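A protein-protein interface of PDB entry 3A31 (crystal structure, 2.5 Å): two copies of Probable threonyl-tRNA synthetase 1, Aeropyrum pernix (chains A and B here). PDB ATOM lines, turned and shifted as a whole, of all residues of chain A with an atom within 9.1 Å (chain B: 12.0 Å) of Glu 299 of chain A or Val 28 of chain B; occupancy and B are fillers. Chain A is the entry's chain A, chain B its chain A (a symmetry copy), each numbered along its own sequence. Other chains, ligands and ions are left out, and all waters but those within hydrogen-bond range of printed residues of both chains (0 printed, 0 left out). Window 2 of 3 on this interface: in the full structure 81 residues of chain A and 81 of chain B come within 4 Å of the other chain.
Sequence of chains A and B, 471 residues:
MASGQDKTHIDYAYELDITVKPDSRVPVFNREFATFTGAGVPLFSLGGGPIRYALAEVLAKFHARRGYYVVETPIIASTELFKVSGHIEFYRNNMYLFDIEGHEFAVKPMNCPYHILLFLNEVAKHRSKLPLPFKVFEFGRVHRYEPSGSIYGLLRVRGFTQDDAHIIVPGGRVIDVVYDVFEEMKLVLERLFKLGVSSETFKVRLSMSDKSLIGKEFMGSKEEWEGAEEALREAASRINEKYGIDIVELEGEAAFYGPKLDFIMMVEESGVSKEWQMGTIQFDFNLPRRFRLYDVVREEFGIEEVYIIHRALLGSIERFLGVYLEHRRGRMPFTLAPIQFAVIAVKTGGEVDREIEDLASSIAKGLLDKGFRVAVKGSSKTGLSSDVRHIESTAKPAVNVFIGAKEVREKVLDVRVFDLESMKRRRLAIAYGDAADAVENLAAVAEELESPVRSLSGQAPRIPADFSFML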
ATOM      1  N   LEU A 120      12.450   7.925 -17.877  1.00  0.00           N
ATOM      2  CA  LEU A 120      13.048   9.051 -17.185  1.00  0.00           C
ATOM      3  C   LEU A 120      12.280  10.328 -17.430  1.00  0.00           C
ATOM      4  O   LEU A 120      12.085  11.125 -16.500  1.00  0.00           O
ATOM      5  CB  LEU A 120      14.521   9.211 -17.539  1.00  0.00           C
ATOM      6  CG  LEU A 120      15.389   8.056 -17.009  1.00  0.00           C
ATOM      7  CD1 LEU A 120      16.778   8.158 -17.550  1.00  0.00           C
ATOM      8  CD2 LEU A 120      15.410   8.018 -15.451  1.00  0.00           C
ATOM      9  N   VAL A 123       9.186  10.188 -15.136  1.00  0.00           N
ATOM     10  CA  VAL A 123       9.540  10.345 -13.747  1.00  0.00           C
ATOM     11  C   VAL A 123       9.741  11.835 -13.481  1.00  0.00           C
ATOM     12  O   VAL A 123       9.163  12.382 -12.553  1.00  0.00           O
ATOM     13  CB  VAL A 123      10.749   9.486 -13.353  1.00  0.00           C
ATOM     14  CG1 VAL A 123      11.329   9.933 -11.975  1.00  0.00           C
ATOM     15  CG2 VAL A 123      10.351   8.038 -13.319  1.00  0.00           C
ATOM     16  N   ALA A 124      10.514  12.502 -14.326  1.00  0.00           N
ATOM     17  CA  ALA A 124      10.738  13.944 -14.176  1.00  0.00           C
ATOM     18  C   ALA A 124       9.467  14.785 -14.092  1.00  0.00           C
ATOM     19  O   ALA A 124       9.413  15.685 -13.311  1.00  0.00           O
ATOM     20  CB  ALA A 124      11.652  14.480 -15.283  1.00  0.00           C
ATOM     21  N   ARG A 127       6.869  12.290 -11.188  1.00  0.00           N
ATOM     22  CA  ARG A 127       7.524  11.562 -10.081  1.00  0.00           C
ATOM     23  C   ARG A 127       6.749  10.320  -9.723  1.00  0.00           C
ATOM     24  O   ARG A 127       6.416   9.511 -10.605  1.00  0.00           O
ATOM     25  CB  ARG A 127       7.752  12.449  -8.861  1.00  0.00           C
ATOM     26  CG  ARG A 127       8.000  13.894  -9.241  1.00  0.00           C
ATOM     27  CD  ARG A 127       8.945  14.670  -8.331  1.00  0.00           C
ATOM     28  NE  ARG A 127       9.669  15.602  -9.209  1.00  0.00           N
ATOM     29  CZ  ARG A 127      10.796  15.309  -9.880  1.00  0.00           C
ATOM     30  NH1 ARG A 127      11.396  14.122  -9.744  1.00  0.00           N
ATOM     31  NH2 ARG A 127      11.345  16.212 -10.687  1.00  0.00           N
ATOM     32  N   SER A 128       6.411  10.189  -8.449  1.00  0.00           N
ATOM     33  CA  SER A 128       5.876   8.912  -7.964  1.00  0.00           C
ATOM     34  C   SER A 128       4.449   8.614  -8.388  1.00  0.00           C
ATOM     35  O   SER A 128       3.953   7.522  -8.073  1.00  0.00           O
ATOM     36  CB  SER A 128       6.035   8.742  -6.443  1.00  0.00           C
ATOM     37  OG  SER A 128       5.567   9.905  -5.803  1.00  0.00           O
ATOM     38  N   PRO A 288      20.039  -0.507 -15.186  1.00  0.00           N
ATOM     39  CA  PRO A 288      19.675   0.281 -13.996  1.00  0.00           C
ATOM     40  C   PRO A 288      20.859   0.999 -13.325  1.00  0.00           C
ATOM     41  O   PRO A 288      20.634   2.005 -12.635  1.00  0.00           O
ATOM     42  CB  PRO A 288      19.101  -0.749 -13.028  1.00  0.00           C
ATOM     43  CG  PRO A 288      19.514  -2.074 -13.522  1.00  0.00           C
ATOM     44  CD  PRO A 288      19.742  -1.940 -15.017  1.00  0.00           C
ATOM     45  N   ARG A 289      22.094   0.499 -13.514  1.00  0.00           N
ATOM     46  CA  ARG A 289      23.314   1.209 -13.097  1.00  0.00           C
ATOM     47  C   ARG A 289      23.686   2.314 -14.096  1.00  0.00           C
ATOM     48  O   ARG A 289      23.958   3.449 -13.723  1.00  0.00           O
ATOM     49  CB  ARG A 289      24.502   0.226 -12.932  1.00  0.00           C
ATOM     50  CG  ARG A 289      24.458  -0.587 -11.596  1.00  0.00           C
ATOM     51  CD  ARG A 289      25.473  -1.714 -11.636  1.00  0.00           C
ATOM     52  NE  ARG A 289      25.622  -2.423 -10.356  1.00  0.00           N
ATOM     53  CZ  ARG A 289      24.923  -3.498  -9.995  1.00  0.00           C
ATOM     54  NH1 ARG A 289      23.976  -4.007 -10.792  1.00  0.00           N
ATOM     55  NH2 ARG A 289      25.163  -4.072  -8.833  1.00  0.00           N
ATOM     56  N   ARG A 290      23.731   1.982 -15.377  1.00  0.00           N
ATOM     57  CA  ARG A 290      24.182   2.964 -16.349  1.00  0.00           C
ATOM     58  C   ARG A 290      23.254   4.200 -16.478  1.00  0.00           C
ATOM     59  O   ARG A 290      23.729   5.307 -16.691  1.00  0.00           O
ATOM     60  CB  ARG A 290      24.413   2.280 -17.684  1.00  0.00           C
ATOM     61  CG  ARG A 290      25.364   1.101 -17.634  1.00  0.00           C
ATOM     62  CD  ARG A 290      26.787   1.527 -17.472  1.00  0.00           C
ATOM     63  NE  ARG A 290      27.127   2.611 -18.393  1.00  0.00           N
ATOM     64  CZ  ARG A 290      28.371   3.078 -18.577  1.00  0.00           C
ATOM     65  NH1 ARG A 290      29.381   2.550 -17.891  1.00  0.00           N
ATOM     66  NH2 ARG A 290      28.610   4.066 -19.436  1.00  0.00           N
ATOM     67  N   PHE A 291      21.946   4.002 -16.322  1.00  0.00           N
ATOM     68  CA  PHE A 291      20.959   5.100 -16.393  1.00  0.00           C
ATOM     69  C   PHE A 291      20.445   5.519 -15.029  1.00  0.00           C
ATOM     70  O   PHE A 291      19.399   6.177 -14.939  1.00  0.00           O
ATOM     71  CB  PHE A 291      19.753   4.672 -17.219  1.00  0.00           C
ATOM     72  CG  PHE A 291      20.000   4.663 -18.693  1.00  0.00           C
ATOM     73  CD1 PHE A 291      19.843   5.832 -19.449  1.00  0.00           C
ATOM     74  CD2 PHE A 291      20.414   3.507 -19.317  1.00  0.00           C
ATOM     75  CE1 PHE A 291      20.059   5.836 -20.810  1.00  0.00           C
ATOM     76  CE2 PHE A 291      20.688   3.492 -20.668  1.00  0.00           C
ATOM     77  CZ  PHE A 291      20.497   4.664 -21.428  1.00  0.00           C
ATOM     78  N   ARG A 292      21.154   5.076 -13.979  1.00  0.00           N
ATOM     79  CA  ARG A 292      20.895   5.411 -12.616  1.00  0.00           C
ATOM     80  C   ARG A 292      19.445   5.164 -12.220  1.00  0.00           C
ATOM     81  O   ARG A 292      18.821   5.976 -11.489  1.00  0.00           O
ATOM     82  CB  ARG A 292      21.391   6.823 -12.328  1.00  0.00           C
ATOM     83  CG  ARG A 292      22.928   6.942 -12.477  1.00  0.00           C
ATOM     84  CD  ARG A 292      23.352   8.397 -12.645  1.00  0.00           C
ATOM     85  NE  ARG A 292      24.719   8.605 -13.174  1.00  0.00           N
ATOM     86  CZ  ARG A 292      25.204   9.795 -13.555  1.00  0.00           C
ATOM     87  NH1 ARG A 292      24.458  10.894 -13.478  1.00  0.00           N
ATOM     88  NH2 ARG A 292      26.436   9.902 -14.028  1.00  0.00           N
ATOM     89  N   LEU A 293      18.921   4.005 -12.629  1.00  0.00           N
ATOM     90  CA  LEU A 293      17.523   3.673 -12.330  1.00  0.00           C
ATOM     91  C   LEU A 293      17.314   3.269 -10.900  1.00  0.00           C
ATOM     92  O   LEU A 293      16.278   3.591 -10.308  1.00  0.00           O
ATOM     93  CB  LEU A 293      16.972   2.624 -13.281  1.00  0.00           C
ATOM     94  CG  LEU A 293      17.163   2.997 -14.773  1.00  0.00           C
ATOM     95  CD1 LEU A 293      16.619   1.885 -15.745  1.00  0.00           C
ATOM     96  CD2 LEU A 293      16.594   4.465 -15.108  1.00  0.00           C
ATOM     97  N   TYR A 294      18.298   2.564 -10.341  1.00  0.00           N
ATOM     98  CA  TYR A 294      18.266   2.201  -8.912  1.00  0.00           C
ATOM     99  C   TYR A 294      18.153   3.451  -8.009  1.00  0.00           C
ATOM    100  O   TYR A 294      17.347   3.478  -7.099  1.00  0.00           O
ATOM    101  CB  TYR A 294      19.493   1.397  -8.546  1.00  0.00           C
ATOM    102  CG  TYR A 294      19.484  -0.015  -9.086  1.00  0.00           C
ATOM    103  CD1 TYR A 294      18.293  -0.743  -9.186  1.00  0.00           C
ATOM    104  CD2 TYR A 294      20.682  -0.645  -9.468  1.00  0.00           C
ATOM    105  CE1 TYR A 294      18.269  -2.058  -9.677  1.00  0.00           C
ATOM    106  CE2 TYR A 294      20.683  -1.975  -9.912  1.00  0.00           C
ATOM    107  CZ  TYR A 294      19.483  -2.666 -10.024  1.00  0.00           C
ATOM    108  OH  TYR A 294      19.497  -3.960 -10.491  1.00  0.00           O
ATOM    109  N   ASP A 295      18.971   4.465  -8.298  1.00  0.00           N
ATOM    110  CA  ASP A 295      18.898   5.716  -7.632  1.00  0.00           C
ATOM    111  C   ASP A 295      17.500   6.302  -7.774  1.00  0.00           C
ATOM    112  O   ASP A 295      16.836   6.591  -6.772  1.00  0.00           O
ATOM    113  CB  ASP A 295      19.933   6.687  -8.197  1.00  0.00           C
ATOM    114  CG  ASP A 295      21.375   6.308  -7.819  1.00  0.00           C
ATOM    115  OD1 ASP A 295      21.592   5.495  -6.875  1.00  0.00           O
ATOM    116  OD2 ASP A 295      22.296   6.836  -8.493  1.00  0.00           O
ATOM    117  N   VAL A 296      17.071   6.479  -9.017  1.00  0.00           N
ATOM    118  CA  VAL A 296      15.829   7.130  -9.336  1.00  0.00           C
ATOM    119  C   VAL A 296      14.645   6.467  -8.647  1.00  0.00           C
ATOM    120  O   VAL A 296      13.793   7.144  -8.126  1.00  0.00           O
ATOM    121  CB  VAL A 296      15.629   7.151 -10.896  1.00  0.00           C
ATOM    122  CG1 VAL A 296      14.183   7.490 -11.266  1.00  0.00           C
ATOM    123  CG2 VAL A 296      16.643   8.084 -11.555  1.00  0.00           C
ATOM    124  N   VAL A 297      14.594   5.143  -8.636  1.00  0.00           N
ATOM    125  CA  VAL A 297      13.458   4.419  -8.045  1.00  0.00           C
ATOM    126  C   VAL A 297      13.454   4.452  -6.511  1.00  0.00           C
ATOM    127  O   VAL A 297      12.384   4.388  -5.869  1.00  0.00           O
ATOM    128  CB  VAL A 297      13.444   2.927  -8.521  1.00  0.00           C
ATOM    129  CG1 VAL A 297      12.337   2.139  -7.863  1.00  0.00           C
ATOM    130  CG2 VAL A 297      13.313   2.880  -9.997  1.00  0.00           C
ATOM    131  N   ARG A 298      14.661   4.464  -5.938  1.00  0.00           N
ATOM    132  CA  ARG A 298      14.846   4.596  -4.498  1.00  0.00           C
ATOM    133  C   ARG A 298      14.451   6.021  -4.089  1.00  0.00           C
ATOM    134  O   ARG A 298      13.566   6.195  -3.250  1.00  0.00           O
ATOM    135  CB  ARG A 298      16.296   4.222  -4.077  1.00  0.00           C
ATOM    136  CG  ARG A 298      16.550   4.125  -2.575  1.00  0.00           C
ATOM    137  CD  ARG A 298      18.049   4.078  -2.247  1.00  0.00           C
ATOM    138  NE  ARG A 298      18.773   5.235  -2.782  1.00  0.00           N
ATOM    139  CZ  ARG A 298      19.704   5.190  -3.739  1.00  0.00           C
ATOM    140  NH1 ARG A 298      20.087   4.028  -4.300  1.00  0.00           N
ATOM    141  NH2 ARG A 298      20.263   6.336  -4.132  1.00  0.00           N
ATOM    142  N   GLU A 299      15.064   7.028  -4.704  1.00  0.00           N
ATOM    143  CA  GLU A 299      14.753   8.417  -4.399  1.00  0.00           C
ATOM    144  C   GLU A 299      13.282   8.825  -4.656  1.00  0.00           C
ATOM    145  O   GLU A 299      12.659   9.431  -3.797  1.00  0.00           O
ATOM    146  CB  GLU A 299      15.699   9.375  -5.120  1.00  0.00           C
ATOM    147  CG  GLU A 299      17.122   9.455  -4.580  1.00  0.00           C
ATOM    148  CD  GLU A 299      18.165   9.913  -5.638  1.00  0.00           C
ATOM    149  OE1 GLU A 299      17.812  10.508  -6.718  1.00  0.00           O
ATOM    150  OE2 GLU A 299      19.373   9.670  -5.385  1.00  0.00           O
ATOM    151  N   GLU A 300      12.708   8.473  -5.798  1.00  0.00           N
ATOM    152  CA  GLU A 300      11.350   8.902  -6.105  1.00  0.00           C
ATOM    153  C   GLU A 300      10.224   8.000  -5.589  1.00  0.00           C
ATOM    154  O   GLU A 300       9.093   8.488  -5.338  1.00  0.00           O
ATOM    155  CB  GLU A 300      11.186   9.095  -7.612  1.00  0.00           C
ATOM    156  CG  GLU A 300      12.103  10.151  -8.210  1.00  0.00           C
ATOM    157  CD  GLU A 300      11.849  11.548  -7.674  1.00  0.00           C
ATOM    158  OE1 GLU A 300      10.767  11.805  -7.054  1.00  0.00           O
ATOM    159  OE2 GLU A 300      12.749  12.404  -7.890  1.00  0.00           O
ATOM    160  N   PHE A 301      10.477   6.697  -5.479  1.00  0.00           N
ATOM    161  CA  PHE A 301       9.399   5.772  -5.069  1.00  0.00           C
ATOM    162  C   PHE A 301       9.662   5.109  -3.727  1.00  0.00           C
ATOM    163  O   PHE A 301       8.805   4.416  -3.203  1.00  0.00           O
ATOM    164  CB  PHE A 301       9.139   4.679  -6.121  1.00  0.00           C
ATOM    165  CG  PHE A 301       8.763   5.193  -7.475  1.00  0.00           C
ATOM    166  CD1 PHE A 301       7.450   5.184  -7.886  1.00  0.00           C
ATOM    167  CD2 PHE A 301       9.736   5.684  -8.345  1.00  0.00           C
ATOM    168  CE1 PHE A 301       7.100   5.671  -9.171  1.00  0.00           C
ATOM    169  CE2 PHE A 301       9.406   6.163  -9.611  1.00  0.00           C
ATOM    170  CZ  PHE A 301       8.078   6.146 -10.037  1.00  0.00           C
ATOM    171  N   GLY A 302      10.856   5.313  -3.181  1.00  0.00           N
ATOM    172  CA  GLY A 302      11.269   4.620  -1.967  1.00  0.00           C
ATOM    173  C   GLY A 302      11.368   3.113  -2.185  1.00  0.00           C
ATOM    174  O   GLY A 302      11.017   2.342  -1.304  1.00  0.00           O
ATOM    175  N   ILE A 303      11.802   2.670  -3.363  1.00  0.00           N
ATOM    176  CA  ILE A 303      11.823   1.235  -3.592  1.00  0.00           C
ATOM    177  C   ILE A 303      13.235   0.761  -3.774  1.00  0.00           C
ATOM    178  O   ILE A 303      13.989   1.312  -4.546  1.00  0.00           O
ATOM    179  CB  ILE A 303      10.889   0.803  -4.753  1.00  0.00           C
ATOM    180  CG1 ILE A 303       9.430   0.935  -4.312  1.00  0.00           C
ATOM    181  CG2 ILE A 303      11.222  -0.621  -5.259  1.00  0.00           C
ATOM    182  CD1 ILE A 303       8.483   0.744  -5.413  1.00  0.00           C
ATOM    183  N   GLU A 304      13.570  -0.283  -3.027  1.00  0.00           N
ATOM    184  CA  GLU A 304      14.941  -0.776  -2.934  1.00  0.00           C
ATOM    185  C   GLU A 304      15.129  -2.005  -3.816  1.00  0.00           C
ATOM    186  O   GLU A 304      16.194  -2.183  -4.445  1.00  0.00           O
ATOM    187  CB  GLU A 304      15.288  -1.105  -1.482  1.00  0.00           C
ATOM    188  CG  GLU A 304      16.665  -0.605  -1.077  1.00  0.00           C
ATOM    189  CD  GLU A 304      16.612   0.688  -0.220  1.00  0.00           C
ATOM    190  OE1 GLU A 304      16.482   0.566   1.024  1.00  0.00           O
ATOM    191  OE2 GLU A 304      16.729   1.813  -0.776  1.00  0.00           O
ATOM    192  N   SER B  24      14.633  19.699 -21.706  1.00  0.00           N
ATOM    193  CA  SER B  24      14.327  19.152 -20.392  1.00  0.00           C
ATOM    194  C   SER B  24      15.578  18.431 -19.896  1.00  0.00           C
ATOM    195  O   SER B  24      16.302  17.771 -20.680  1.00  0.00           O
ATOM    196  CB  SER B  24      13.212  18.113 -20.466  1.00  0.00           C
ATOM    197  OG  SER B  24      11.997  18.677 -20.891  1.00  0.00           O
ATOM    198  N   ARG B  25      15.818  18.563 -18.598  1.00  0.00           N
ATOM    199  CA  ARG B  25      16.910  17.869 -17.920  1.00  0.00           C
ATOM    200  C   ARG B  25      16.559  16.407 -17.553  1.00  0.00           C
ATOM    201  O   ARG B  25      15.513  16.137 -16.938  1.00  0.00           O
ATOM    202  CB  ARG B  25      17.267  18.601 -16.622  1.00  0.00           C
ATOM    203  CG  ARG B  25      17.800  19.989 -16.816  1.00  0.00           C
ATOM    204  CD  ARG B  25      19.315  20.017 -17.027  1.00  0.00           C
ATOM    205  NE  ARG B  25      19.756  21.359 -17.399  1.00  0.00           N
ATOM    206  CZ  ARG B  25      21.008  21.693 -17.741  1.00  0.00           C
ATOM    207  NH1 ARG B  25      21.999  20.779 -17.775  1.00  0.00           N
ATOM    208  NH2 ARG B  25      21.274  22.967 -18.059  1.00  0.00           N
ATOM    209  N   VAL B  26      17.469  15.485 -17.847  1.00  0.00           N
ATOM    210  CA  VAL B  26      17.299  14.093 -17.422  1.00  0.00           C
ATOM    211  C   VAL B  26      17.473  13.922 -15.913  1.00  0.00           C
ATOM    212  O   VAL B  26      18.479  14.334 -15.359  1.00  0.00           O
ATOM    213  CB  VAL B  26      18.206  13.170 -18.237  1.00  0.00           C
ATOM    214  CG1 VAL B  26      18.002  11.677 -17.849  1.00  0.00           C
ATOM    215  CG2 VAL B  26      17.913  13.393 -19.757  1.00  0.00           C
ATOM    216  N   PRO B  27      16.472  13.348 -15.221  1.00  0.00           N
ATOM    217  CA  PRO B  27      16.672  13.187 -13.756  1.00  0.00           C
ATOM    218  C   PRO B  27      18.026  12.538 -13.401  1.00  0.00           C
ATOM    219  O   PRO B  27      18.538  11.689 -14.141  1.00  0.00           O
ATOM    220  CB  PRO B  27      15.542  12.248 -13.330  1.00  0.00           C
ATOM    221  CG  PRO B  27      14.509  12.362 -14.392  1.00  0.00           C
ATOM    222  CD  PRO B  27      15.178  12.807 -15.681  1.00  0.00           C
ATOM    223  N   VAL B  28      18.578  12.929 -12.259  1.00  0.00           N
ATOM    224  CA  VAL B  28      19.858  12.426 -11.749  1.00  0.00           C
ATOM    225  C   VAL B  28      21.054  12.810 -12.624  1.00  0.00           C
ATOM    226  O   VAL B  28      22.025  13.323 -12.099  1.00  0.00           O
ATOM    227  CB  VAL B  28      19.880  10.916 -11.367  1.00  0.00           C
ATOM    228  CG1 VAL B  28      21.206  10.589 -10.679  1.00  0.00           C
ATOM    229  CG2 VAL B  28      18.739  10.561 -10.414  1.00  0.00           C
ATOM    230  N   PHE B  29      21.019  12.632 -13.938  1.00  0.00           N
ATOM    231  CA  PHE B  29      22.099  13.191 -14.735  1.00  0.00           C
ATOM    232  C   PHE B  29      22.180  14.724 -14.767  1.00  0.00           C
ATOM    233  O   PHE B  29      23.232  15.255 -15.077  1.00  0.00           O
ATOM    234  CB  PHE B  29      21.985  12.735 -16.169  1.00  0.00           C
ATOM    235  CG  PHE B  29      22.178  11.285 -16.357  1.00  0.00           C
ATOM    236  CD1 PHE B  29      23.436  10.776 -16.661  1.00  0.00           C
ATOM    237  CD2 PHE B  29      21.116  10.420 -16.243  1.00  0.00           C
ATOM    238  CE1 PHE B  29      23.630   9.412 -16.846  1.00  0.00           C
ATOM    239  CE2 PHE B  29      21.294   9.071 -16.443  1.00  0.00           C
ATOM    240  CZ  PHE B  29      22.564   8.558 -16.747  1.00  0.00           C
ATOM    241  N   ASN B  30      21.089  15.441 -14.495  1.00  0.00           N
ATOM    242  CA  ASN B  30      20.946  16.840 -15.032  1.00  0.00           C
ATOM    243  C   ASN B  30      21.744  17.198 -16.379  1.00  0.00           C
ATOM    244  O   ASN B  30      22.716  17.985 -16.433  1.00  0.00           O
ATOM    245  CB  ASN B  30      21.078  17.921 -13.916  1.00  0.00           C
ATOM    246  CG  ASN B  30      20.061  17.716 -12.739  1.00  0.00           C
ATOM    247  OD1 ASN B  30      18.967  17.108 -12.899  1.00  0.00           O
ATOM    248  ND2 ASN B  30      20.427  18.238 -11.555  1.00  0.00           N
ATOM    249  N   ARG B  31      21.339  16.566 -17.467  1.00  0.00           N
ATOM    250  CA  ARG B  31      21.749  17.012 -18.771  1.00  0.00           C
ATOM    251  C   ARG B  31      20.465  16.986 -19.572  1.00  0.00           C
ATOM    252  O   ARG B  31      19.501  16.306 -19.207  1.00  0.00           O
ATOM    253  CB  ARG B  31      22.759  16.065 -19.365  1.00  0.00           C
ATOM    254  CG  ARG B  31      23.871  15.689 -18.423  1.00  0.00           C
ATOM    255  CD  ARG B  31      24.869  14.784 -19.196  1.00  0.00           C
ATOM    256  NE  ARG B  31      25.437  13.672 -18.400  1.00  0.00           N
ATOM    257  CZ  ARG B  31      25.842  12.500 -18.920  1.00  0.00           C
ATOM    258  NH1 ARG B  31      25.745  12.263 -20.232  1.00  0.00           N
ATOM    259  NH2 ARG B  31      26.336  11.547 -18.132  1.00  0.00           N
ATOM    260  N   GLU B  32      20.435  17.749 -20.646  1.00  0.00           N
ATOM    261  CA  GLU B  32      19.268  17.784 -21.509  1.00  0.00           C
ATOM    262  C   GLU B  32      19.050  16.451 -22.219  1.00  0.00           C
ATOM    263  O   GLU B  32      20.014  15.708 -22.445  1.00  0.00           O
ATOM    264  CB  GLU B  32      19.442  18.909 -22.489  1.00  0.00           C
ATOM    265  CG  GLU B  32      19.571  20.189 -21.729  1.00  0.00           C
ATOM    266  CD  GLU B  32      19.566  21.402 -22.603  1.00  0.00           C
ATOM    267  OE1 GLU B  32      19.870  21.281 -23.822  1.00  0.00           O
ATOM    268  OE2 GLU B  32      19.225  22.468 -22.039  1.00  0.00           O
ATOM    269  N   PHE B  33      17.792  16.129 -22.552  1.00  0.00           N
ATOM    270  CA  PHE B  33      17.523  14.891 -23.287  1.00  0.00           C
ATOM    271  C   PHE B  33      18.298  14.915 -24.592  1.00  0.00           C
ATOM    272  O   PHE B  33      18.825  13.880 -25.020  1.00  0.00           O
ATOM    273  CB  PHE B  33      16.037  14.597 -23.458  1.00  0.00           C
ATOM    274  CG  PHE B  33      15.380  13.953 -22.234  1.00  0.00           C
ATOM    275  CD1 PHE B  33      15.243  12.576 -22.143  1.00  0.00           C
ATOM    276  CD2 PHE B  33      14.898  14.744 -21.172  1.00  0.00           C
ATOM    277  CE1 PHE B  33      14.648  11.976 -21.028  1.00  0.00           C
ATOM    278  CE2 PHE B  33      14.319  14.182 -20.057  1.00  0.00           C
ATOM    279  CZ  PHE B  33      14.178  12.806 -19.972  1.00  0.00           C
ATOM    280  N   THR B  35      21.256  16.013 -25.292  1.00  0.00           N
ATOM    281  CA  THR B  35      22.653  15.612 -25.264  1.00  0.00           C
ATOM    282  C   THR B  35      22.802  14.073 -25.287  1.00  0.00           C
ATOM    283  O   THR B  35      23.940  13.583 -25.254  1.00  0.00           O
ATOM    284  CB  THR B  35      23.460  16.209 -24.075  1.00  0.00           C
ATOM    285  OG1 THR B  35      23.065  15.557 -22.874  1.00  0.00           O
ATOM    286  CG2 THR B  35      23.227  17.750 -23.907  1.00  0.00           C
ATOM    287  N   PHE B  36      21.671  13.332 -25.329  1.00  0.00           N
ATOM    288  CA  PHE B  36      21.676  11.874 -25.463  1.00  0.00           C
ATOM    289  C   PHE B  36      21.221  11.508 -26.847  1.00  0.00           C
ATOM    290  O   PHE B  36      21.690  10.513 -27.403  1.00  0.00           O
ATOM    291  CB  PHE B  36      20.703  11.176 -24.538  1.00  0.00           C
ATOM    292  CG  PHE B  36      21.006  11.282 -23.070  1.00  0.00           C
ATOM    293  CD1 PHE B  36      21.232  10.127 -22.319  1.00  0.00           C
ATOM    294  CD2 PHE B  36      20.972  12.505 -22.404  1.00  0.00           C
ATOM    295  CE1 PHE B  36      21.451  10.185 -20.942  1.00  0.00           C
ATOM    296  CE2 PHE B  36      21.197  12.570 -21.022  1.00  0.00           C
ATOM    297  CZ  PHE B  36      21.436  11.402 -20.296  1.00  0.00           C
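Printed residues of chain B that touch a printed residue of chain A: Val 26, Pro 27, Val 28 and Phe 29. Hydrophobic or aromatic side chains of chain A that line the printed part of chain B: Leu 120, Ala 124 and Val 296. Among the printed residues, 9 pairs touch across the chains. Among the printed residues, no Asp or Glu carboxylate lies within 4 Å of a Lys or Arg side-chain nitrogen of the other chain.
No position is printed for both chains. Of the 9 pairs that touch across the chains among the printed residues, none has its exchanged pair printed and touching as well.
Printed residues of chain B within 4 Å of Ala 124 of chain A: Pro 27 (3.7 Å). Of the printed residues of chain B, Arg 290 of chain A touches Phe 29. Of the printed residues of chain B, Phe 291 of chain A touches Phe 29 (3.8 Å). Printed residues of chain B within 4 Å of Arg 292 of chain A: Val 28 and Phe 29. Val 296 of chain A touches just one residue of chain B: Val 28. Of chain B, only Val 28 (3.8 Å) comes within 4 Å of Glu 299 of chain A. Phe 301 of chain A touches none of the printed residues of chain B. No residue of chain B comes within 4 Å of Gly 302 of chain A. Printed residues of chain A within 4 Å of Val 26 of chain B: Leu 120 (3.7 Å). Pro 27 of chain B touches just these residues of chain A: Leu 120 and Ala 124. Of chain A, only Arg 292, Val 296 and Glu 299 come within 4 Å of Val 28 of chain B. The nearest residue of chain A that does not touch Val 28 of chain B is Asp 295 of chain A (4.5 Å).
The backbone carbonyl oxygen of Ala 124 of chain A sits at hydrogen-bond distance from the guanidinium group of Arg 127 of chain A, 3.3 Å away. O of Arg 31 of chain B sits at hydrogen-bond distance from N of Val 26 of chain B (2.6 Å). NH2 of Arg 298 of chain A lies within salt-bridge range of OE2 of Glu 299 of chain A.
CD1 of Leu 120 of chain A touches CG1 of Val 26 of chain B, at 3.7 Å. CG of Pro 27 of chain B touches O of Leu 120 of chain A, 3.4 Å away. Ala 124 of chain A touches Pro 27 of chain B. Phe 29 of chain B touches Arg 290 of chain A. O of Phe 291 of chain A touches CE2 of Phe 29 of chain B (3.8 Å). Arg 292 of chain A touches Val 28 of chain B. NH1 of Arg 292 of chain A touches CD1 of Phe 29 of chain B (3.3 Å). Val 28 of chain B touches Val 296 of chain A. Val 28 of chain B touches Glu 299 of chain A (CG2 to OE1, 3.8 Å).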
